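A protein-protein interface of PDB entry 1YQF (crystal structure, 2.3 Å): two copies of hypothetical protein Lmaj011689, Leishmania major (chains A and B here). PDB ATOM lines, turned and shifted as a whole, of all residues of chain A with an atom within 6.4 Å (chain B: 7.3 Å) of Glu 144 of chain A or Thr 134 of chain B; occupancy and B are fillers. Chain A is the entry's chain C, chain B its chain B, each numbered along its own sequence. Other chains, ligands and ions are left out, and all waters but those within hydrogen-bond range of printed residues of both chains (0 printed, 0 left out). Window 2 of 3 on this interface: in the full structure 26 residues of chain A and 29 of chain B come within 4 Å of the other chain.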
ATOM      1  N   ARG A 123       6.738 -21.688  21.810  1.00  0.00           N
ATOM      2  CA  ARG A 123       7.655 -21.521  20.681  1.00  0.00           C
ATOM      3  C   ARG A 123       8.808 -22.517  20.723  1.00  0.00           C
ATOM      4  O   ARG A 123       9.049 -23.158  21.742  1.00  0.00           O
ATOM      5  CB  ARG A 123       8.208 -20.098  20.654  1.00  0.00           C
ATOM      6  CG  ARG A 123       8.923 -19.681  21.921  1.00  0.00           C
ATOM      7  CD  ARG A 123       9.287 -18.218  21.950  1.00  0.00           C
ATOM      8  NE  ARG A 123      10.161 -17.886  20.829  1.00  0.00           N
ATOM      9  CZ  ARG A 123      10.672 -16.687  20.597  1.00  0.00           C
ATOM     10  NH1 ARG A 123      10.408 -15.672  21.409  1.00  0.00           N
ATOM     11  NH2 ARG A 123      11.464 -16.502  19.553  1.00  0.00           N
ATOM     12  N   GLU A 137      21.562  -9.126  23.597  1.00  0.00           N
ATOM     13  CA  GLU A 137      21.754  -9.494  22.199  1.00  0.00           C
ATOM     14  C   GLU A 137      21.082 -10.823  21.892  1.00  0.00           C
ATOM     15  O   GLU A 137      20.618 -11.033  20.780  1.00  0.00           O
ATOM     16  CB  GLU A 137      23.244  -9.553  21.835  1.00  0.00           C
ATOM     17  CG  GLU A 137      23.910  -8.194  21.641  1.00  0.00           C
ATOM     18  CD  GLU A 137      23.227  -7.318  20.601  1.00  0.00           C
ATOM     19  OE1 GLU A 137      22.512  -7.855  19.728  1.00  0.00           O
ATOM     20  OE2 GLU A 137      23.404  -6.084  20.658  1.00  0.00           O
ATOM     21  N   GLU A 139      18.261 -11.886  23.466  1.00  0.00           N
ATOM     22  CA  GLU A 139      16.840 -11.554  23.393  1.00  0.00           C
ATOM     23  C   GLU A 139      16.491 -10.958  22.033  1.00  0.00           C
ATOM     24  O   GLU A 139      15.431 -11.238  21.485  1.00  0.00           O
ATOM     25  CB  GLU A 139      16.444 -10.574  24.496  1.00  0.00           C
ATOM     26  CG  GLU A 139      14.936 -10.414  24.649  1.00  0.00           C
ATOM     27  CD  GLU A 139      14.550  -9.192  25.458  1.00  0.00           C
ATOM     28  OE1 GLU A 139      14.828  -8.062  25.003  1.00  0.00           O
ATOM     29  OE2 GLU A 139      13.961  -9.362  26.544  1.00  0.00           O
ATOM     30  N   ALA A 140      17.388 -10.132  21.501  1.00  0.00           N
ATOM     31  CA  ALA A 140      17.200  -9.520  20.190  1.00  0.00           C
ATOM     32  C   ALA A 140      17.146 -10.587  19.100  1.00  0.00           C
ATOM     33  O   ALA A 140      16.346 -10.481  18.173  1.00  0.00           O
ATOM     34  CB  ALA A 140      18.313  -8.529  19.904  1.00  0.00           C
ATOM     35  N   LYS A 141      17.993 -11.611  19.230  1.00  0.00           N
ATOM     36  CA  LYS A 141      17.994 -12.761  18.321  1.00  0.00           C
ATOM     37  C   LYS A 141      16.634 -13.451  18.360  1.00  0.00           C
ATOM     38  O   LYS A 141      16.009 -13.675  17.322  1.00  0.00           O
ATOM     39  CB  LYS A 141      19.053 -13.798  18.726  1.00  0.00           C
ATOM     40  CG  LYS A 141      20.511 -13.370  18.651  1.00  0.00           C
ATOM     41  CD  LYS A 141      21.394 -14.378  19.419  1.00  0.00           C
ATOM     42  CE  LYS A 141      22.841 -13.907  19.548  1.00  0.00           C
ATOM     43  NZ  LYS A 141      23.517 -14.342  20.812  1.00  0.00           N
ATOM     44  N   ARG A 142      16.195 -13.789  19.574  1.00  0.00           N
ATOM     45  CA  ARG A 142      14.912 -14.454  19.805  1.00  0.00           C
ATOM     46  C   ARG A 142      13.727 -13.627  19.294  1.00  0.00           C
ATOM     47  O   ARG A 142      12.770 -14.185  18.771  1.00  0.00           O
ATOM     48  CB  ARG A 142      14.728 -14.760  21.298  1.00  0.00           C
ATOM     49  CG  ARG A 142      15.641 -15.858  21.847  1.00  0.00           C
ATOM     50  CD  ARG A 142      15.188 -16.414  23.194  1.00  0.00           C
ATOM     51  NE  ARG A 142      15.099 -15.362  24.201  1.00  0.00           N
ATOM     52  CZ  ARG A 142      16.094 -14.954  24.987  1.00  0.00           C
ATOM     53  NH1 ARG A 142      17.292 -15.522  24.925  1.00  0.00           N
ATOM     54  NH2 ARG A 142      15.884 -13.967  25.855  1.00  0.00           N
ATOM     55  N   ASN A 143      13.808 -12.302  19.422  1.00  0.00           N
ATOM     56  CA  ASN A 143      12.744 -11.400  18.966  1.00  0.00           C
ATOM     57  C   ASN A 143      12.514 -11.460  17.456  1.00  0.00           C
ATOM     58  O   ASN A 143      11.428 -11.127  16.979  1.00  0.00           O
ATOM     59  CB  ASN A 143      13.059  -9.942  19.341  1.00  0.00           C
ATOM     60  CG  ASN A 143      12.763  -9.624  20.804  1.00  0.00           C
ATOM     61  OD1 ASN A 143      12.115 -10.394  21.513  1.00  0.00           O
ATOM     62  ND2 ASN A 143      13.241  -8.471  21.258  1.00  0.00           N
ATOM     63  N   GLU A 144      13.539 -11.863  16.710  1.00  0.00           N
ATOM     64  CA  GLU A 144      13.444 -11.971  15.258  1.00  0.00           C
ATOM     65  C   GLU A 144      12.721 -13.246  14.825  1.00  0.00           C
ATOM     66  O   GLU A 144      12.122 -13.284  13.754  1.00  0.00           O
ATOM     67  CB  GLU A 144      14.844 -11.954  14.632  1.00  0.00           C
ATOM     68  CG  GLU A 144      15.552 -10.610  14.690  1.00  0.00           C
ATOM     69  CD  GLU A 144      16.852 -10.607  13.904  1.00  0.00           C
ATOM     70  OE1 GLU A 144      17.803 -11.304  14.321  1.00  0.00           O
ATOM     71  OE2 GLU A 144      16.923  -9.915  12.865  1.00  0.00           O
ATOM     72  N   LEU A 145      12.794 -14.291  15.648  1.00  0.00           N
ATOM     73  CA  LEU A 145      12.235 -15.594  15.285  1.00  0.00           C
ATOM     74  C   LEU A 145      10.724 -15.666  15.471  1.00  0.00           C
ATOM     75  O   LEU A 145      10.111 -14.788  16.079  1.00  0.00           O
ATOM     76  CB  LEU A 145      12.912 -16.713  16.082  1.00  0.00           C
ATOM     77  CG  LEU A 145      14.446 -16.680  16.133  1.00  0.00           C
ATOM     78  CD1 LEU A 145      14.985 -17.962  16.751  1.00  0.00           C
ATOM     79  CD2 LEU A 145      15.056 -16.456  14.749  1.00  0.00           C
ATOM     80  N   TYR A 146      10.139 -16.728  14.923  1.00  0.00           N
ATOM     81  CA  TYR A 146       8.707 -16.980  15.012  1.00  0.00           C
ATOM     82  C   TYR A 146       8.318 -17.334  16.450  1.00  0.00           C
ATOM     83  O   TYR A 146       8.741 -18.355  16.976  1.00  0.00           O
ATOM     84  CB  TYR A 146       8.324 -18.120  14.062  1.00  0.00           C
ATOM     85  CG  TYR A 146       6.879 -18.559  14.155  1.00  0.00           C
ATOM     86  CD1 TYR A 146       5.842 -17.665  13.912  1.00  0.00           C
ATOM     87  CD2 TYR A 146       6.552 -19.868  14.485  1.00  0.00           C
ATOM     88  CE1 TYR A 146       4.515 -18.067  13.993  1.00  0.00           C
ATOM     89  CE2 TYR A 146       5.230 -20.278  14.569  1.00  0.00           C
ATOM     90  CZ  TYR A 146       4.217 -19.375  14.324  1.00  0.00           C
ATOM     91  OH  TYR A 146       2.901 -19.779  14.408  1.00  0.00           O
ATOM     92  N   LYS B  59      15.313 -12.256   6.069  1.00  0.00           N
ATOM     93  CA  LYS B  59      16.581 -12.381   6.777  1.00  0.00           C
ATOM     94  C   LYS B  59      16.702 -13.845   7.213  1.00  0.00           C
ATOM     95  O   LYS B  59      15.870 -14.319   7.983  1.00  0.00           O
ATOM     96  CB  LYS B  59      16.596 -11.440   7.986  1.00  0.00           C
ATOM     97  CG  LYS B  59      17.943 -11.281   8.669  1.00  0.00           C
ATOM     98  CD  LYS B  59      17.955 -10.030   9.543  1.00  0.00           C
ATOM     99  CE  LYS B  59      19.238  -9.900  10.347  1.00  0.00           C
ATOM    100  NZ  LYS B  59      19.230 -10.771  11.556  1.00  0.00           N
ATOM    101  N   PRO B  60      17.709 -14.560   6.704  1.00  0.00           N
ATOM    102  CA  PRO B  60      17.844 -16.018   6.907  1.00  0.00           C
ATOM    103  C   PRO B  60      17.439 -16.551   8.292  1.00  0.00           C
ATOM    104  O   PRO B  60      18.105 -16.280   9.294  1.00  0.00           O
ATOM    105  CB  PRO B  60      19.336 -16.253   6.644  1.00  0.00           C
ATOM    106  CG  PRO B  60      19.650 -15.265   5.563  1.00  0.00           C
ATOM    107  CD  PRO B  60      18.824 -14.038   5.884  1.00  0.00           C
ATOM    108  N   GLY B  61      16.343 -17.309   8.326  1.00  0.00           N
ATOM    109  CA  GLY B  61      15.880 -17.966   9.541  1.00  0.00           C
ATOM    110  C   GLY B  61      15.029 -17.110  10.467  1.00  0.00           C
ATOM    111  O   GLY B  61      14.893 -17.440  11.646  1.00  0.00           O
ATOM    112  N   THR B  62      14.443 -16.034   9.938  1.00  0.00           N
ATOM    113  CA  THR B  62      13.633 -15.113  10.740  1.00  0.00           C
ATOM    114  C   THR B  62      12.278 -14.842  10.094  1.00  0.00           C
ATOM    115  O   THR B  62      11.973 -15.335   9.008  1.00  0.00           O
ATOM    116  CB  THR B  62      14.365 -13.760  10.962  1.00  0.00           C
ATOM    117  OG1 THR B  62      14.400 -13.010   9.740  1.00  0.00           O
ATOM    118  CG2 THR B  62      15.834 -13.950  11.332  1.00  0.00           C
ATOM    119  N   CYS B  63      11.477 -14.040  10.788  1.00  0.00           N
ATOM    120  CA  CYS B  63      10.180 -13.587  10.303  1.00  0.00           C
ATOM    121  C   CYS B  63      10.244 -12.127   9.849  1.00  0.00           C
ATOM    122  O   CYS B  63       9.220 -11.459   9.737  1.00  0.00           O
ATOM    123  CB  CYS B  63       9.147 -13.751  11.416  1.00  0.00           C
ATOM    124  SG  CYS B  63       8.752 -15.475  11.728  1.00  0.00           S
ATOM    125  N   THR B  64      11.451 -11.637   9.587  1.00  0.00           N
ATOM    126  CA  THR B  64      11.653 -10.267   9.138  1.00  0.00           C
ATOM    127  C   THR B  64      11.788 -10.264   7.624  1.00  0.00           C
ATOM    128  O   THR B  64      12.553 -11.053   7.067  1.00  0.00           O
ATOM    129  CB  THR B  64      12.916  -9.684   9.783  1.00  0.00           C
ATOM    130  OG1 THR B  64      12.733  -9.584  11.201  1.00  0.00           O
ATOM    131  CG2 THR B  64      13.162  -8.243   9.331  1.00  0.00           C
ATOM    132  N   ARG B  79      10.419  -2.570   5.687  1.00  0.00           N
ATOM    133  CA  ARG B  79      10.606  -3.704   6.583  1.00  0.00           C
ATOM    134  C   ARG B  79       9.368  -3.965   7.425  1.00  0.00           C
ATOM    135  O   ARG B  79       8.761  -3.044   7.962  1.00  0.00           O
ATOM    136  CB  ARG B  79      11.804  -3.452   7.498  1.00  0.00           C
ATOM    137  CG  ARG B  79      12.051  -4.547   8.534  1.00  0.00           C
ATOM    138  CD  ARG B  79      13.381  -4.418   9.243  1.00  0.00           C
ATOM    139  NE  ARG B  79      14.493  -4.433   8.294  1.00  0.00           N
ATOM    140  CZ  ARG B  79      15.756  -4.161   8.595  1.00  0.00           C
ATOM    141  NH1 ARG B  79      16.101  -3.850   9.832  1.00  0.00           N
ATOM    142  NH2 ARG B  79      16.687  -4.205   7.648  1.00  0.00           N
ATOM    143  N   SER B  81       7.721  -7.398  10.080  1.00  0.00           N
ATOM    144  CA  SER B  81       7.789  -8.766  10.589  1.00  0.00           C
ATOM    145  C   SER B  81       6.461  -9.460  10.308  1.00  0.00           C
ATOM    146  O   SER B  81       5.415  -8.811  10.259  1.00  0.00           O
ATOM    147  CB  SER B  81       8.085  -8.782  12.087  1.00  0.00           C
ATOM    148  OG  SER B  81       8.101 -10.112  12.581  1.00  0.00           O
ATOM    149  N   THR B  82       6.510 -10.779  10.136  1.00  0.00           N
ATOM    150  CA  THR B  82       5.316 -11.573   9.849  1.00  0.00           C
ATOM    151  C   THR B  82       4.795 -12.282  11.102  1.00  0.00           C
ATOM    152  O   THR B  82       4.031 -13.247  11.009  1.00  0.00           O
ATOM    153  CB  THR B  82       5.592 -12.582   8.711  1.00  0.00           C
ATOM    154  OG1 THR B  82       4.387 -13.309   8.418  1.00  0.00           O
ATOM    155  CG2 THR B  82       6.610 -13.660   9.108  1.00  0.00           C
ATOM    156  N   ASN B  83       5.208 -11.789  12.268  1.00  0.00           N
ATOM    157  CA  ASN B  83       4.777 -12.325  13.548  1.00  0.00           C
ATOM    158  C   ASN B  83       3.658 -11.483  14.141  1.00  0.00           C
ATOM    159  O   ASN B  83       3.598 -10.273  13.923  1.00  0.00           O
ATOM    160  CB  ASN B  83       5.951 -12.357  14.521  1.00  0.00           C
ATOM    161  CG  ASN B  83       5.915 -13.568  15.425  1.00  0.00           C
ATOM    162  OD1 ASN B  83       4.913 -13.844  16.100  1.00  0.00           O
ATOM    163  ND2 ASN B  83       7.010 -14.309  15.436  1.00  0.00           N
ATOM    164  N   TYR B  97      12.814   2.767   5.107  1.00  0.00           N
ATOM    165  CA  TYR B  97      14.128   3.396   5.116  1.00  0.00           C
ATOM    166  C   TYR B  97      14.480   3.899   3.718  1.00  0.00           C
ATOM    167  O   TYR B  97      14.406   3.145   2.754  1.00  0.00           O
ATOM    168  CB  TYR B  97      15.186   2.397   5.581  1.00  0.00           C
ATOM    169  CG  TYR B  97      14.871   1.755   6.914  1.00  0.00           C
ATOM    170  CD1 TYR B  97      15.154   2.417   8.108  1.00  0.00           C
ATOM    171  CD2 TYR B  97      14.297   0.489   6.984  1.00  0.00           C
ATOM    172  CE1 TYR B  97      14.878   1.838   9.329  1.00  0.00           C
ATOM    173  CE2 TYR B  97      14.010  -0.101   8.212  1.00  0.00           C
ATOM    174  CZ  TYR B  97      14.304   0.581   9.379  1.00  0.00           C
ATOM    175  OH  TYR B  97      14.027   0.015  10.600  1.00  0.00           O
ATOM    176  N   ALA B 129      23.420   2.196   8.371  1.00  0.00           N
ATOM    177  CA  ALA B 129      23.730   1.114   9.301  1.00  0.00           C
ATOM    178  C   ALA B 129      22.936   1.268  10.592  1.00  0.00           C
ATOM    179  O   ALA B 129      22.114   0.420  10.920  1.00  0.00           O
ATOM    180  CB  ALA B 129      25.216   1.072   9.598  1.00  0.00           C
ATOM    181  N   LEU B 130      23.159   2.371  11.302  1.00  0.00           N
ATOM    182  CA  LEU B 130      22.467   2.632  12.564  1.00  0.00           C
ATOM    183  C   LEU B 130      20.948   2.462  12.458  1.00  0.00           C
ATOM    184  O   LEU B 130      20.308   2.030  13.408  1.00  0.00           O
ATOM    185  CB  LEU B 130      22.798   4.039  13.071  1.00  0.00           C
ATOM    186  CG  LEU B 130      22.036   4.531  14.308  1.00  0.00           C
ATOM    187  CD1 LEU B 130      22.234   3.594  15.500  1.00  0.00           C
ATOM    188  CD2 LEU B 130      22.472   5.941  14.655  1.00  0.00           C
ATOM    189  N   ALA B 131      20.377   2.799  11.305  1.00  0.00           N
ATOM    190  CA  ALA B 131      18.928   2.722  11.105  1.00  0.00           C
ATOM    191  C   ALA B 131      18.402   1.293  10.908  1.00  0.00           C
ATOM    192  O   ALA B 131      17.426   0.896  11.543  1.00  0.00           O
ATOM    193  CB  ALA B 131      18.530   3.585   9.920  1.00  0.00           C
ATOM    194  N   LYS B 132      19.044   0.539  10.018  1.00  0.00           N
ATOM    195  CA  LYS B 132      18.576  -0.792   9.623  1.00  0.00           C
ATOM    196  C   LYS B 132      19.099  -1.895  10.537  1.00  0.00           C
ATOM    197  O   LYS B 132      18.505  -2.961  10.644  1.00  0.00           O
ATOM    198  CB  LYS B 132      18.984  -1.086   8.175  1.00  0.00           C
ATOM    199  CG  LYS B 132      18.416  -0.093   7.166  1.00  0.00           C
ATOM    200  CD  LYS B 132      19.023  -0.261   5.781  1.00  0.00           C
ATOM    201  CE  LYS B 132      18.648   0.908   4.875  1.00  0.00           C
ATOM    202  NZ  LYS B 132      19.348   0.884   3.559  1.00  0.00           N
ATOM    203  N   ASP B 133      20.218  -1.635  11.195  1.00  0.00           N
ATOM    204  CA  ASP B 133      20.842  -2.611  12.083  1.00  0.00           C
ATOM    205  C   ASP B 133      19.840  -3.129  13.123  1.00  0.00           C
ATOM    206  O   ASP B 133      19.335  -2.357  13.934  1.00  0.00           O
ATOM    207  CB  ASP B 133      22.049  -1.966  12.775  1.00  0.00           C
ATOM    208  CG  ASP B 133      23.016  -2.978  13.330  1.00  0.00           C
ATOM    209  OD1 ASP B 133      22.618  -3.750  14.219  1.00  0.00           O
ATOM    210  OD2 ASP B 133      24.201  -3.062  12.947  1.00  0.00           O
ATOM    211  N   THR B 134      19.527  -4.427  13.070  1.00  0.00           N
ATOM    212  CA  THR B 134      18.815  -5.077  14.178  1.00  0.00           C
ATOM    213  C   THR B 134      19.868  -5.394  15.225  1.00  0.00           C
ATOM    214  O   THR B 134      21.059  -5.195  14.990  1.00  0.00           O
ATOM    215  CB  THR B 134      18.091  -6.373  13.733  1.00  0.00           C
ATOM    216  OG1 THR B 134      19.041  -7.342  13.250  1.00  0.00           O
ATOM    217  CG2 THR B 134      17.170  -6.120  12.545  1.00  0.00           C
ATOM    218  N   GLY B 135      19.452  -5.902  16.373  1.00  0.00           N
ATOM    219  CA  GLY B 135      20.389  -6.113  17.465  1.00  0.00           C
ATOM    220  C   GLY B 135      20.086  -5.147  18.591  1.00  0.00           C
ATOM    221  O   GLY B 135      19.677  -4.012  18.357  1.00  0.00           O
ATOM    222  N   ALA B 136      20.273  -5.625  19.816  1.00  0.00           N
ATOM    223  CA  ALA B 136      19.892  -4.901  21.022  1.00  0.00           C
ATOM    224  C   ALA B 136      20.600  -3.559  21.175  1.00  0.00           C
ATOM    225  O   ALA B 136      19.972  -2.564  21.525  1.00  0.00           O
ATOM    226  CB  ALA B 136      20.153  -5.771  22.233  1.00  0.00           C
ATOM    227  N   GLU B 137      21.903  -3.538  20.910  1.00  0.00           N
ATOM    228  CA  GLU B 137      22.709  -2.336  21.108  1.00  0.00           C
ATOM    229  C   GLU B 137      22.343  -1.240  20.113  1.00  0.00           C
ATOM    230  O   GLU B 137      22.285  -0.062  20.472  1.00  0.00           O
ATOM    231  CB  GLU B 137      24.205  -2.662  21.014  1.00  0.00           C
ATOM    232  CG  GLU B 137      25.080  -1.872  21.974  1.00  0.00           C
ATOM    233  CD  GLU B 137      24.611  -1.953  23.418  1.00  0.00           C
ATOM    234  OE1 GLU B 137      24.681  -3.045  24.025  1.00  0.00           O
ATOM    235  OE2 GLU B 137      24.166  -0.911  23.942  1.00  0.00           O
ATOM    236  N   ALA B 138      22.100  -1.631  18.865  1.00  0.00           N
ATOM    237  CA  ALA B 138      21.682  -0.688  17.834  1.00  0.00           C
ATOM    238  C   ALA B 138      20.356  -0.034  18.205  1.00  0.00           C
ATOM    239  O   ALA B 138      20.177   1.170  18.004  1.00  0.00           O
ATOM    240  CB  ALA B 138      21.572  -1.385  16.487  1.00  0.00           C
ATOM    241  N   GLU B 139      19.436  -0.825  18.757  1.00  0.00           N
ATOM    242  CA  GLU B 139      18.128  -0.315  19.166  1.00  0.00           C
ATOM    243  C   GLU B 139      18.272   0.679  20.318  1.00  0.00           C
ATOM    244  O   GLU B 139      17.581   1.696  20.347  1.00  0.00           O
ATOM    245  CB  GLU B 139      17.191  -1.463  19.564  1.00  0.00           C
ATOM    246  CG  GLU B 139      15.717  -1.071  19.684  1.00  0.00           C
ATOM    247  CD  GLU B 139      15.051  -0.772  18.344  1.00  0.00           C
ATOM    248  OE1 GLU B 139      15.091  -1.642  17.439  1.00  0.00           O
ATOM    249  OE2 GLU B 139      14.473   0.330  18.192  1.00  0.00           O
ATOM    250  N   ARG B 142      19.355   4.021  19.065  1.00  0.00           N
ATOM    251  CA  ARG B 142      18.215   4.674  18.425  1.00  0.00           C
ATOM    252  C   ARG B 142      17.262   5.292  19.459  1.00  0.00           C
ATOM    253  O   ARG B 142      16.791   6.406  19.271  1.00  0.00           O
ATOM    254  CB  ARG B 142      17.454   3.690  17.533  1.00  0.00           C
ATOM    255  CG  ARG B 142      18.129   3.387  16.206  1.00  0.00           C
ATOM    256  CD  ARG B 142      17.194   2.748  15.179  1.00  0.00           C
ATOM    257  NE  ARG B 142      16.835   1.375  15.541  1.00  0.00           N
ATOM    258  CZ  ARG B 142      17.645   0.325  15.428  1.00  0.00           C
ATOM    259  NH1 ARG B 142      18.875   0.469  14.957  1.00  0.00           N
ATOM    260  NH2 ARG B 142      17.222  -0.879  15.789  1.00  0.00           N
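The backbone NH (N) of Ala 136 of chain B lies within hydrogen-bond range of the side-chain carboxylate (OE1) of Glu 137 of chain A, at 3.2 Å. O of Leu 145 of chain A sits at hydrogen-bond distance from ND2 of Asn 83 of chain B, 3.2 Å away. O of Glu 144 of chain A sits at hydrogen-bond distance from N of Cys 63 of chain B (3.1 Å). The side-chain sulfur (SG) of Cys 63 of chain B lies close to the backbone NH (N) of Tyr 146 of chain A, at 3.7 Å. The side-chain hydroxyl of Thr 134 of chain B is in hydrogen-bond range of the side-chain carboxylate of Glu 144 of chain A, at 3.4 Å. The side-chain carboxylate of Glu 144 of chain A is in salt-bridge range of the side-chain amino group of Lys 59 of chain B (2.8 Å). OE2 of Glu 137 of chain A is in hydrogen-bond range of N of Glu 137 of chain B.
OG of Ser 81 of chain B lies close to O of Cys 63 of chain B, at 3.3 Å. The side-chain hydroxyl of Thr 62 of chain B is in hydrogen-bond range of the backbone NH of Thr 64 of chain B, at 3.3 Å. The side-chain hydroxyl (OG) of Ser 81 of chain B lies close to the backbone NH (N) of Asn 83 of chain B, at 3.4 Å. N of Thr 82 of chain B lies within hydrogen-bond range of O of Cys 63 of chain B. The backbone NH (N) of Lys 59 of chain B lies within hydrogen-bond range of the backbone carbonyl oxygen (O) of Thr 64 of chain B (3.2 Å). The backbone carbonyl oxygen (O) of Lys 59 of chain B sits at hydrogen-bond distance from the side-chain hydroxyl (OG1) of Thr 62 of chain B, 2.6 Å away.
Among the printed residues, pairs that only touch across the chains: Tyr 146 of chain A with Asn 83 of chain B, Leu 145 of chain A with Gly 61 of chain B, Ala 140 of chain A with Ala 136 of chain B, Glu 137 of chain A with Gly 135 of chain B and Glu 144 of chain A with Thr 62 of chain B.
Printed residues of chain B within 4 Å of Glu 144 of chain A: Lys 59 (2.8 Å), Thr 62 (3.6 Å), Cys 63 (3.1 Å) and Thr 134 (3.4 Å). Of the printed residues of chain A, Thr 134 of chain B touches Glu 144 (3.4 Å). Of the printed residues of chain B, Leu 145 of chain A touches Gly 61 (3.3 Å) and Asn 83 (3.2 Å). Of the printed residues of chain A, Glu 137 of chain B touches Glu 137 (3.0 Å). Of the printed residues of chain B, Glu 137 of chain A touches Gly 135 (3.6 Å), Ala 136 (3.2 Å) and Glu 137 (3.0 Å). Of the printed residues of chain A, Lys 59 of chain B touches Glu 144. The nearest residue of chain B that does not touch Glu 144 of chain A is Thr 64 of chain B (4.5 Å). The nearest residue of chain A that does not touch Thr 134 of chain B is Glu 137 of chain A (5.6 Å). The nearest printed residue of chain B that does not touch Leu 145 of chain A is Cys 63 of chain B (4.2 Å).
Of the 23 printed residues of chain B, 9 touch a printed residue of chain A. Printed residues of chain B that touch a printed residue of chain A: Lys 59, Gly 61, Thr 62, Cys 63, Asn 83, Thr 134, Gly 135, Ala 136 and Glu 137. Among the printed residues, Asp or Glu carboxylates within 4 Å of a Lys or Arg side-chain nitrogen of the other chain: Glu 144 of chain A with Lys 59 of chain B (2.8 Å).
Glu 137 of chain B touches its own counterpart, Glu 137 of chain A. Positions printed for both chains: 137, 139 and 142.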
